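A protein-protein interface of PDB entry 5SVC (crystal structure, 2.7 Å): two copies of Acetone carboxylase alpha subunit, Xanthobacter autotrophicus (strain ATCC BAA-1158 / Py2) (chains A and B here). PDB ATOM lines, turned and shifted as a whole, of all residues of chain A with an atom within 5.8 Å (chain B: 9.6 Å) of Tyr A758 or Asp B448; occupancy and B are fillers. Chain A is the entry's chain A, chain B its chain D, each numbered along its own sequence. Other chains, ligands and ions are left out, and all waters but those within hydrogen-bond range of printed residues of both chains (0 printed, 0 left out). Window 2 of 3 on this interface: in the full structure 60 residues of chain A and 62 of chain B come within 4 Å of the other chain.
N of Gly A755 lies within hydrogen-bond range of OD2 of Asp B531 (2.7 Å). SD of Met A760 lies close to N of Ile B450 (3.7 Å).
The backbone carbonyl oxygen of Asn B445 sits at hydrogen-bond distance from the side-chain amino group of Lys B530 (3.2 Å). The side-chain carboxylate (OD1) of Asp B448 is in salt-bridge range of the side-chain amino group (NZ) of Lys B530 (3.1 Å). O of Lys B530 sits at hydrogen-bond distance from N of Phe B444. The side-chain amide oxygen (OD1) of Asn B445 sits at hydrogen-bond distance from the backbone NH (N) of Asp B448, 3.2 Å away. N of Met A760 sits at hydrogen-bond distance from OD1 of Asp A392 (3.3 Å). OD2 of Asp A392 lies within salt-bridge range of NE of Arg A394 (3.1 Å).
Among the printed residues, pairs that only touch across the chains: Arg A394 with Phe B444 (3.1 Å), Tyr A758 with Asp B448 (3.4 Å), Arg A394 with Ile B450 (3.4 Å), Tyr A758 with Lys B530 (3.4 Å), Ser A759 with Phe B444 (3.5 Å), Tyr A758 with Phe B444 (3.8 Å) and Met A760 with Phe B444 (3.9 Å).
Gly A755 touches just one residue of chain B: Asp B531 (2.7 Å). Of chain B, only Phe B444, Asp B448 and Lys B530 come within 4 Å of Tyr A758. Of the printed residues of chain A, Phe B444 touches Arg A394 (3.1 Å), Tyr A758 (3.8 Å), Ser A759 (3.5 Å) and Met A760 (3.9 Å). Printed residues of chain A within 4 Å of Asp B448: Tyr A758. His B451 touches none of the printed residues of chain A. Printed residues of chain A within 4 Å of Lys B530: Tyr A758. Trp B532 touches none of the printed residues of chain A. The nearest residue of chain B that does not touch Tyr A758 is Asp B531 (4.2 Å). The nearest residue of chain A that does not touch Asp B448 is Ser A759 (5.4 Å).
Of the 9 printed residues of chain A, 5 touch a printed residue of chain B. Printed residues of chain A that touch a printed residue of chain B: Arg A394, Gly A755, Tyr A758, Ser A759 and Met A760. Among the printed residues, no Asp or Glu carboxylate lies within 4 Å of a Lys or Arg side-chain nitrogen of the other chain.
No position is printed for both chains.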
ATOM      1  N   TRP A 340       0.796  33.763 -24.552  1.00  0.00           N
ATOM      2  CA  TRP A 340       1.631  34.486 -23.610  1.00  0.00           C
ATOM      3  C   TRP A 340       2.730  33.578 -23.074  1.00  0.00           C
ATOM      4  O   TRP A 340       2.649  32.356 -23.135  1.00  0.00           O
ATOM      5  CB  TRP A 340       0.790  35.011 -22.457  1.00  0.00           C
ATOM      6  CG  TRP A 340       0.008  33.964 -21.782  1.00  0.00           C
ATOM      7  CD1 TRP A 340      -1.272  33.579 -22.087  1.00  0.00           C
ATOM      8  CD2 TRP A 340       0.412  33.153 -20.665  1.00  0.00           C
ATOM      9  NE1 TRP A 340      -1.696  32.593 -21.218  1.00  0.00           N
ATOM     10  CE2 TRP A 340      -0.680  32.305 -20.344  1.00  0.00           C
ATOM     11  CE3 TRP A 340       1.571  33.074 -19.894  1.00  0.00           C
ATOM     12  CZ2 TRP A 340      -0.636  31.381 -19.303  1.00  0.00           C
ATOM     13  CZ3 TRP A 340       1.609  32.148 -18.853  1.00  0.00           C
ATOM     14  CH2 TRP A 340       0.503  31.318 -18.570  1.00  0.00           C
ATOM     15  N   ASP A 392      -4.270  34.929 -17.885  1.00  0.00           N
ATOM     16  CA  ASP A 392      -3.482  34.577 -16.715  1.00  0.00           C
ATOM     17  C   ASP A 392      -3.066  35.824 -15.944  1.00  0.00           C
ATOM     18  O   ASP A 392      -2.649  36.828 -16.539  1.00  0.00           O
ATOM     19  CB  ASP A 392      -2.255  33.764 -17.114  1.00  0.00           C
ATOM     20  CG  ASP A 392      -1.692  33.006 -15.946  1.00  0.00           C
ATOM     21  OD1 ASP A 392      -2.269  31.921 -15.653  1.00  0.00           O
ATOM     22  OD2 ASP A 392      -0.692  33.486 -15.330  1.00  0.00           O
ATOM     23  N   ARG A 394      -0.682  35.913 -13.598  1.00  0.00           N
ATOM     24  CA  ARG A 394       0.746  35.914 -13.286  1.00  0.00           C
ATOM     25  C   ARG A 394       1.608  36.618 -14.335  1.00  0.00           C
ATOM     26  O   ARG A 394       2.752  36.983 -14.040  1.00  0.00           O
ATOM     27  CB  ARG A 394       1.216  34.484 -13.107  1.00  0.00           C
ATOM     28  CG  ARG A 394       0.631  33.831 -11.867  1.00  0.00           C
ATOM     29  CD  ARG A 394       0.854  32.325 -11.850  1.00  0.00           C
ATOM     30  NE  ARG A 394       0.160  31.642 -12.938  1.00  0.00           N
ATOM     31  CZ  ARG A 394       0.487  30.427 -13.357  1.00  0.00           C
ATOM     32  NH1 ARG A 394       1.499  29.789 -12.782  1.00  0.00           N
ATOM     33  NH2 ARG A 394      -0.181  29.850 -14.346  1.00  0.00           N
ATOM     34  N   GLY A 755       1.974  26.604 -18.164  1.00  0.00           N
ATOM     35  CA  GLY A 755       0.934  27.514 -18.599  1.00  0.00           C
ATOM     36  C   GLY A 755       0.341  27.261 -19.979  1.00  0.00           C
ATOM     37  O   GLY A 755      -0.213  28.184 -20.584  1.00  0.00           O
ATOM     38  N   SER A 756       0.460  26.060 -20.525  1.00  0.00           N
ATOM     39  CA  SER A 756      -0.129  25.828 -21.842  1.00  0.00           C
ATOM     40  C   SER A 756      -1.568  25.325 -21.753  1.00  0.00           C
ATOM     41  O   SER A 756      -2.354  25.569 -22.675  1.00  0.00           O
ATOM     42  CB  SER A 756       0.704  24.826 -22.644  1.00  0.00           C
ATOM     43  OG  SER A 756       0.545  23.524 -22.098  1.00  0.00           O
ATOM     44  N   ARG A 757      -1.919  24.633 -20.665  1.00  0.00           N
ATOM     45  CA  ARG A 757      -3.278  24.189 -20.395  1.00  0.00           C
ATOM     46  C   ARG A 757      -3.900  24.903 -19.199  1.00  0.00           C
ATOM     47  O   ARG A 757      -5.020  25.411 -19.310  1.00  0.00           O
ATOM     48  CB  ARG A 757      -3.295  22.675 -20.180  1.00  0.00           C
ATOM     49  CG  ARG A 757      -2.166  21.986 -20.926  1.00  0.00           C
ATOM     50  CD  ARG A 757      -2.446  20.514 -21.239  1.00  0.00           C
ATOM     51  NE  ARG A 757      -3.538  20.379 -22.205  1.00  0.00           N
ATOM     52  CZ  ARG A 757      -3.431  20.650 -23.506  1.00  0.00           C
ATOM     53  NH1 ARG A 757      -2.275  21.077 -24.009  1.00  0.00           N
ATOM     54  NH2 ARG A 757      -4.486  20.500 -24.306  1.00  0.00           N
ATOM     55  N   TYR A 758      -3.201  24.992 -18.064  1.00  0.00           N
ATOM     56  CA  TYR A 758      -3.769  25.573 -16.848  1.00  0.00           C
ATOM     57  C   TYR A 758      -3.507  27.072 -16.775  1.00  0.00           C
ATOM     58  O   TYR A 758      -2.379  27.520 -16.994  1.00  0.00           O
ATOM     59  CB  TYR A 758      -3.218  24.870 -15.606  1.00  0.00           C
ATOM     60  CG  TYR A 758      -3.717  23.431 -15.488  1.00  0.00           C
ATOM     61  CD1 TYR A 758      -3.071  22.383 -16.155  1.00  0.00           C
ATOM     62  CD2 TYR A 758      -4.842  23.122 -14.713  1.00  0.00           C
ATOM     63  CE1 TYR A 758      -3.540  21.083 -16.052  1.00  0.00           C
ATOM     64  CE2 TYR A 758      -5.317  21.816 -14.596  1.00  0.00           C
ATOM     65  CZ  TYR A 758      -4.669  20.808 -15.264  1.00  0.00           C
ATOM     66  OH  TYR A 758      -5.147  19.523 -15.134  1.00  0.00           O
ATOM     67  N   SER A 759      -4.548  27.841 -16.434  1.00  0.00           N
ATOM     68  CA  SER A 759      -4.436  29.289 -16.324  1.00  0.00           C
ATOM     69  C   SER A 759      -5.565  29.802 -15.437  1.00  0.00           C
ATOM     70  O   SER A 759      -6.606  29.157 -15.311  1.00  0.00           O
ATOM     71  CB  SER A 759      -4.481  29.958 -17.702  1.00  0.00           C
ATOM     72  OG  SER A 759      -5.791  29.871 -18.254  1.00  0.00           O
ATOM     73  N   MET A 760      -5.342  30.971 -14.817  1.00  0.00           N
ATOM     74  CA  MET A 760      -6.307  31.606 -13.918  1.00  0.00           C
ATOM     75  C   MET A 760      -6.306  33.090 -14.247  1.00  0.00           C
ATOM     76  O   MET A 760      -5.246  33.712 -14.346  1.00  0.00           O
ATOM     77  CB  MET A 760      -5.979  31.341 -12.433  1.00  0.00           C
ATOM     78  CG  MET A 760      -6.706  32.184 -11.369  1.00  0.00           C
ATOM     79  SD  MET A 760      -6.448  31.602  -9.649  1.00  0.00           S
ATOM     80  CE  MET A 760      -8.059  32.007  -9.010  1.00  0.00           C
ATOM     81  N   ARG B 228      -7.220  33.682  -1.533  1.00  0.00           N
ATOM     82  CA  ARG B 228      -8.220  33.360  -0.509  1.00  0.00           C
ATOM     83  C   ARG B 228      -7.597  33.266   0.881  1.00  0.00           C
ATOM     84  O   ARG B 228      -8.182  33.726   1.867  1.00  0.00           O
ATOM     85  CB  ARG B 228      -8.964  32.053  -0.812  1.00  0.00           C
ATOM     86  CG  ARG B 228     -10.236  32.173  -1.640  1.00  0.00           C
ATOM     87  CD  ARG B 228     -10.657  30.837  -2.273  1.00  0.00           C
ATOM     88  NE  ARG B 228      -9.520  30.089  -2.801  1.00  0.00           N
ATOM     89  CZ  ARG B 228      -8.918  29.081  -2.172  1.00  0.00           C
ATOM     90  NH1 ARG B 228      -9.338  28.670  -0.972  1.00  0.00           N
ATOM     91  NH2 ARG B 228      -7.888  28.482  -2.745  1.00  0.00           N
ATOM     92  N   GLY B 443       2.554  26.880  -8.027  1.00  0.00           N
ATOM     93  CA  GLY B 443       1.936  26.441  -9.273  1.00  0.00           C
ATOM     94  C   GLY B 443       0.419  26.310  -9.111  1.00  0.00           C
ATOM     95  O   GLY B 443      -0.213  27.115  -8.422  1.00  0.00           O
ATOM     96  N   PHE B 444      -0.140  25.296  -9.764  1.00  0.00           N
ATOM     97  CA  PHE B 444      -1.550  24.972  -9.624  1.00  0.00           C
ATOM     98  C   PHE B 444      -1.722  23.818  -8.654  1.00  0.00           C
ATOM     99  O   PHE B 444      -0.999  22.820  -8.736  1.00  0.00           O
ATOM    100  CB  PHE B 444      -2.158  24.619 -10.966  1.00  0.00           C
ATOM    101  CG  PHE B 444      -2.589  25.795 -11.723  1.00  0.00           C
ATOM    102  CD1 PHE B 444      -1.681  26.521 -12.467  1.00  0.00           C
ATOM    103  CD2 PHE B 444      -3.921  26.182 -11.705  1.00  0.00           C
ATOM    104  CE1 PHE B 444      -2.082  27.633 -13.175  1.00  0.00           C
ATOM    105  CE2 PHE B 444      -4.339  27.302 -12.419  1.00  0.00           C
ATOM    106  CZ  PHE B 444      -3.409  28.035 -13.152  1.00  0.00           C
ATOM    107  N   ASN B 445      -2.676  23.966  -7.741  1.00  0.00           N
ATOM    108  CA  ASN B 445      -2.922  23.000  -6.689  1.00  0.00           C
ATOM    109  C   ASN B 445      -4.073  22.064  -7.083  1.00  0.00           C
ATOM    110  O   ASN B 445      -4.568  22.097  -8.209  1.00  0.00           O
ATOM    111  CB  ASN B 445      -3.198  23.767  -5.408  1.00  0.00           C
ATOM    112  CG  ASN B 445      -4.371  24.707  -5.554  1.00  0.00           C
ATOM    113  OD1 ASN B 445      -5.282  24.507  -6.386  1.00  0.00           O
ATOM    114  ND2 ASN B 445      -4.368  25.741  -4.741  1.00  0.00           N
ATOM    115  N   GLN B 446      -4.535  21.247  -6.131  1.00  0.00           N
ATOM    116  CA  GLN B 446      -5.553  20.237  -6.419  1.00  0.00           C
ATOM    117  C   GLN B 446      -6.925  20.838  -6.702  1.00  0.00           C
ATOM    118  O   GLN B 446      -7.776  20.151  -7.264  1.00  0.00           O
ATOM    119  CB  GLN B 446      -5.667  19.247  -5.256  1.00  0.00           C
ATOM    120  CG  GLN B 446      -5.980  19.898  -3.917  1.00  0.00           C
ATOM    121  CD  GLN B 446      -4.742  20.158  -3.054  1.00  0.00           C
ATOM    122  OE1 GLN B 446      -3.800  20.867  -3.468  1.00  0.00           O
ATOM    123  NE2 GLN B 446      -4.762  19.615  -1.818  1.00  0.00           N
ATOM    124  N   TYR B 447      -7.169  22.081  -6.311  1.00  0.00           N
ATOM    125  CA  TYR B 447      -8.383  22.801  -6.683  1.00  0.00           C
ATOM    126  C   TYR B 447      -8.214  23.599  -7.985  1.00  0.00           C
ATOM    127  O   TYR B 447      -9.085  24.403  -8.335  1.00  0.00           O
ATOM    128  CB  TYR B 447      -8.799  23.723  -5.534  1.00  0.00           C
ATOM    129  CG  TYR B 447      -8.611  23.055  -4.198  1.00  0.00           C
ATOM    130  CD1 TYR B 447      -9.430  22.002  -3.805  1.00  0.00           C
ATOM    131  CD2 TYR B 447      -7.587  23.442  -3.347  1.00  0.00           C
ATOM    132  CE1 TYR B 447      -9.247  21.363  -2.590  1.00  0.00           C
ATOM    133  CE2 TYR B 447      -7.399  22.813  -2.118  1.00  0.00           C
ATOM    134  CZ  TYR B 447      -8.228  21.773  -1.746  1.00  0.00           C
ATOM    135  OH  TYR B 447      -8.040  21.143  -0.531  1.00  0.00           O
ATOM    136  N   ASP B 448      -7.114  23.393  -8.696  1.00  0.00           N
ATOM    137  CA  ASP B 448      -6.877  24.032  -9.980  1.00  0.00           C
ATOM    138  C   ASP B 448      -6.839  25.557  -9.874  1.00  0.00           C
ATOM    139  O   ASP B 448      -7.233  26.280 -10.795  1.00  0.00           O
ATOM    140  CB  ASP B 448      -7.907  23.550 -10.995  1.00  0.00           C
ATOM    141  CG  ASP B 448      -7.839  22.042 -11.202  1.00  0.00           C
ATOM    142  OD1 ASP B 448      -6.753  21.542 -11.554  1.00  0.00           O
ATOM    143  OD2 ASP B 448      -8.861  21.353 -11.004  1.00  0.00           O
ATOM    144  N   GLU B 449      -6.308  26.045  -8.754  1.00  0.00           N
ATOM    145  CA  GLU B 449      -6.021  27.457  -8.558  1.00  0.00           C
ATOM    146  C   GLU B 449      -4.522  27.694  -8.384  1.00  0.00           C
ATOM    147  O   GLU B 449      -3.806  26.856  -7.832  1.00  0.00           O
ATOM    148  CB  GLU B 449      -6.752  28.013  -7.330  1.00  0.00           C
ATOM    149  CG  GLU B 449      -8.236  28.086  -7.457  1.00  0.00           C
ATOM    150  CD  GLU B 449      -8.871  28.591  -6.172  1.00  0.00           C
ATOM    151  OE1 GLU B 449      -8.246  28.414  -5.101  1.00  0.00           O
ATOM    152  OE2 GLU B 449      -9.971  29.192  -6.235  1.00  0.00           O
ATOM    153  N   ILE B 450      -4.064  28.854  -8.879  1.00  0.00           N
ATOM    154  CA  ILE B 450      -2.754  29.391  -8.530  1.00  0.00           C
ATOM    155  C   ILE B 450      -2.537  29.325  -7.029  1.00  0.00           C
ATOM    156  O   ILE B 450      -3.429  29.646  -6.233  1.00  0.00           O
ATOM    157  CB  ILE B 450      -2.649  30.851  -8.996  1.00  0.00           C
ATOM    158  CG1 ILE B 450      -2.891  30.978 -10.483  1.00  0.00           C
ATOM    159  CG2 ILE B 450      -1.312  31.462  -8.605  1.00  0.00           C
ATOM    160  CD1 ILE B 450      -2.512  32.306 -10.967  1.00  0.00           C
ATOM    161  N   HIS B 451      -1.333  28.946  -6.631  1.00  0.00           N
ATOM    162  CA  HIS B 451      -1.113  28.593  -5.236  1.00  0.00           C
ATOM    163  C   HIS B 451       0.385  28.578  -4.949  1.00  0.00           C
ATOM    164  O   HIS B 451       1.217  28.479  -5.860  1.00  0.00           O
ATOM    165  CB  HIS B 451      -1.747  27.236  -4.956  1.00  0.00           C
ATOM    166  CG  HIS B 451      -1.767  26.820  -3.522  1.00  0.00           C
ATOM    167  ND1 HIS B 451      -2.515  27.468  -2.566  1.00  0.00           N
ATOM    168  CD2 HIS B 451      -1.185  25.768  -2.897  1.00  0.00           C
ATOM    169  CE1 HIS B 451      -2.375  26.849  -1.405  1.00  0.00           C
ATOM    170  NE2 HIS B 451      -1.569  25.818  -1.578  1.00  0.00           N
ATOM    171  N   PRO B 496      -0.599  20.327  -2.613  1.00  0.00           N
ATOM    172  CA  PRO B 496      -0.758  19.187  -3.533  1.00  0.00           C
ATOM    173  C   PRO B 496       0.394  18.181  -3.426  1.00  0.00           C
ATOM    174  O   PRO B 496       1.161  17.969  -4.369  1.00  0.00           O
ATOM    175  CB  PRO B 496      -0.827  19.883  -4.899  1.00  0.00           C
ATOM    176  CG  PRO B 496       0.063  21.110  -4.737  1.00  0.00           C
ATOM    177  CD  PRO B 496      -0.134  21.548  -3.303  1.00  0.00           C
ATOM    178  N   TRP B 527       1.476  15.444  -5.614  1.00  0.00           N
ATOM    179  CA  TRP B 527       0.231  14.787  -5.987  1.00  0.00           C
ATOM    180  C   TRP B 527      -0.829  15.814  -6.350  1.00  0.00           C
ATOM    181  O   TRP B 527      -1.144  16.685  -5.542  1.00  0.00           O
ATOM    182  CB  TRP B 527      -0.264  13.902  -4.839  1.00  0.00           C
ATOM    183  CG  TRP B 527      -1.527  13.231  -5.158  1.00  0.00           C
ATOM    184  CD1 TRP B 527      -2.761  13.470  -4.612  1.00  0.00           C
ATOM    185  CD2 TRP B 527      -1.713  12.233  -6.149  1.00  0.00           C
ATOM    186  NE1 TRP B 527      -3.699  12.648  -5.183  1.00  0.00           N
ATOM    187  CE2 TRP B 527      -3.083  11.884  -6.140  1.00  0.00           C
ATOM    188  CE3 TRP B 527      -0.855  11.597  -7.050  1.00  0.00           C
ATOM    189  CZ2 TRP B 527      -3.608  10.922  -6.992  1.00  0.00           C
ATOM    190  CZ3 TRP B 527      -1.375  10.648  -7.891  1.00  0.00           C
ATOM    191  CH2 TRP B 527      -2.743  10.319  -7.860  1.00  0.00           C
ATOM    192  N   ASN B 528      -1.395  15.693  -7.549  1.00  0.00           N
ATOM    193  CA  ASN B 528      -2.486  16.548  -7.989  1.00  0.00           C
ATOM    194  C   ASN B 528      -1.996  17.974  -8.195  1.00  0.00           C
ATOM    195  O   ASN B 528      -2.759  18.947  -8.037  1.00  0.00           O
ATOM    196  CB  ASN B 528      -3.644  16.505  -6.988  1.00  0.00           C
ATOM    197  CG  ASN B 528      -5.012  16.639  -7.632  1.00  0.00           C
ATOM    198  OD1 ASN B 528      -5.215  17.368  -8.606  1.00  0.00           O
ATOM    199  ND2 ASN B 528      -5.972  15.919  -7.073  1.00  0.00           N
ATOM    200  N   ALA B 529      -0.719  18.103  -8.563  1.00  0.00           N
ATOM    201  CA  ALA B 529      -0.161  19.410  -8.871  1.00  0.00           C
ATOM    202  C   ALA B 529      -0.062  19.608 -10.379  1.00  0.00           C
ATOM    203  O   ALA B 529       0.014  18.649 -11.141  1.00  0.00           O
ATOM    204  CB  ALA B 529       1.213  19.584  -8.210  1.00  0.00           C
ATOM    205  N   LYS B 530      -0.114  20.859 -10.814  1.00  0.00           N
ATOM    206  CA  LYS B 530       0.091  21.171 -12.224  1.00  0.00           C
ATOM    207  C   LYS B 530       1.033  22.364 -12.357  1.00  0.00           C
ATOM    208  O   LYS B 530       0.923  23.342 -11.611  1.00  0.00           O
ATOM    209  CB  LYS B 530      -1.236  21.469 -12.948  1.00  0.00           C
ATOM    210  CG  LYS B 530      -2.310  20.387 -12.815  1.00  0.00           C
ATOM    211  CD  LYS B 530      -3.160  20.611 -11.557  1.00  0.00           C
ATOM    212  CE  LYS B 530      -4.289  19.641 -11.500  1.00  0.00           C
ATOM    213  NZ  LYS B 530      -4.832  19.521 -10.134  1.00  0.00           N
ATOM    214  N   ASP B 531       1.928  22.295 -13.332  1.00  0.00           N
ATOM    215  CA  ASP B 531       2.871  23.374 -13.592  1.00  0.00           C
ATOM    216  C   ASP B 531       3.562  23.801 -12.294  1.00  0.00           C
ATOM    217  O   ASP B 531       3.567  24.967 -11.907  1.00  0.00           O
ATOM    218  CB  ASP B 531       2.178  24.556 -14.286  1.00  0.00           C
ATOM    219  CG  ASP B 531       1.747  24.237 -15.709  1.00  0.00           C
ATOM    220  OD1 ASP B 531       2.257  23.258 -16.268  1.00  0.00           O
ATOM    221  OD2 ASP B 531       0.946  24.988 -16.299  1.00  0.00           O
ATOM    222  N   TRP B 532       4.180  22.816 -11.652  1.00  0.00           N
ATOM    223  CA  TRP B 532       4.580  22.852 -10.255  1.00  0.00           C
ATOM    224  C   TRP B 532       6.094  22.968 -10.070  1.00  0.00           C
ATOM    225  O   TRP B 532       6.874  22.279 -10.747  1.00  0.00           O
ATOM    226  CB  TRP B 532       4.090  21.575  -9.582  1.00  0.00           C
ATOM    227  CG  TRP B 532       4.232  21.613  -8.127  1.00  0.00           C
ATOM    228  CD1 TRP B 532       5.085  20.880  -7.354  1.00  0.00           C
ATOM    229  CD2 TRP B 532       3.532  22.491  -7.237  1.00  0.00           C
ATOM    230  NE1 TRP B 532       4.919  21.220  -6.028  1.00  0.00           N
ATOM    231  CE2 TRP B 532       3.971  22.203  -5.936  1.00  0.00           C
ATOM    232  CE3 TRP B 532       2.550  23.474  -7.417  1.00  0.00           C
ATOM    233  CZ2 TRP B 532       3.469  22.855  -4.835  1.00  0.00           C
ATOM    234  CZ3 TRP B 532       2.055  24.115  -6.323  1.00  0.00           C
ATOM    235  CH2 TRP B 532       2.520  23.820  -5.051  1.00  0.00           C
ATOM    236  N   ASP B 614       3.929  15.126 -10.749  1.00  0.00           N
ATOM    237  CA  ASP B 614       3.258  14.157  -9.901  1.00  0.00           C
ATOM    238  C   ASP B 614       4.109  12.891  -9.844  1.00  0.00           C
ATOM    239  O   ASP B 614       4.577  12.395 -10.878  1.00  0.00           O
ATOM    240  CB  ASP B 614       1.842  13.868 -10.423  1.00  0.00           C
ATOM    241  CG  ASP B 614       0.797  14.854  -9.877  1.00  0.00           C
ATOM    242  OD1 ASP B 614       1.228  15.909  -9.371  1.00  0.00           O
ATOM    243  OD2 ASP B 614      -0.435  14.590  -9.968  1.00  0.00           O
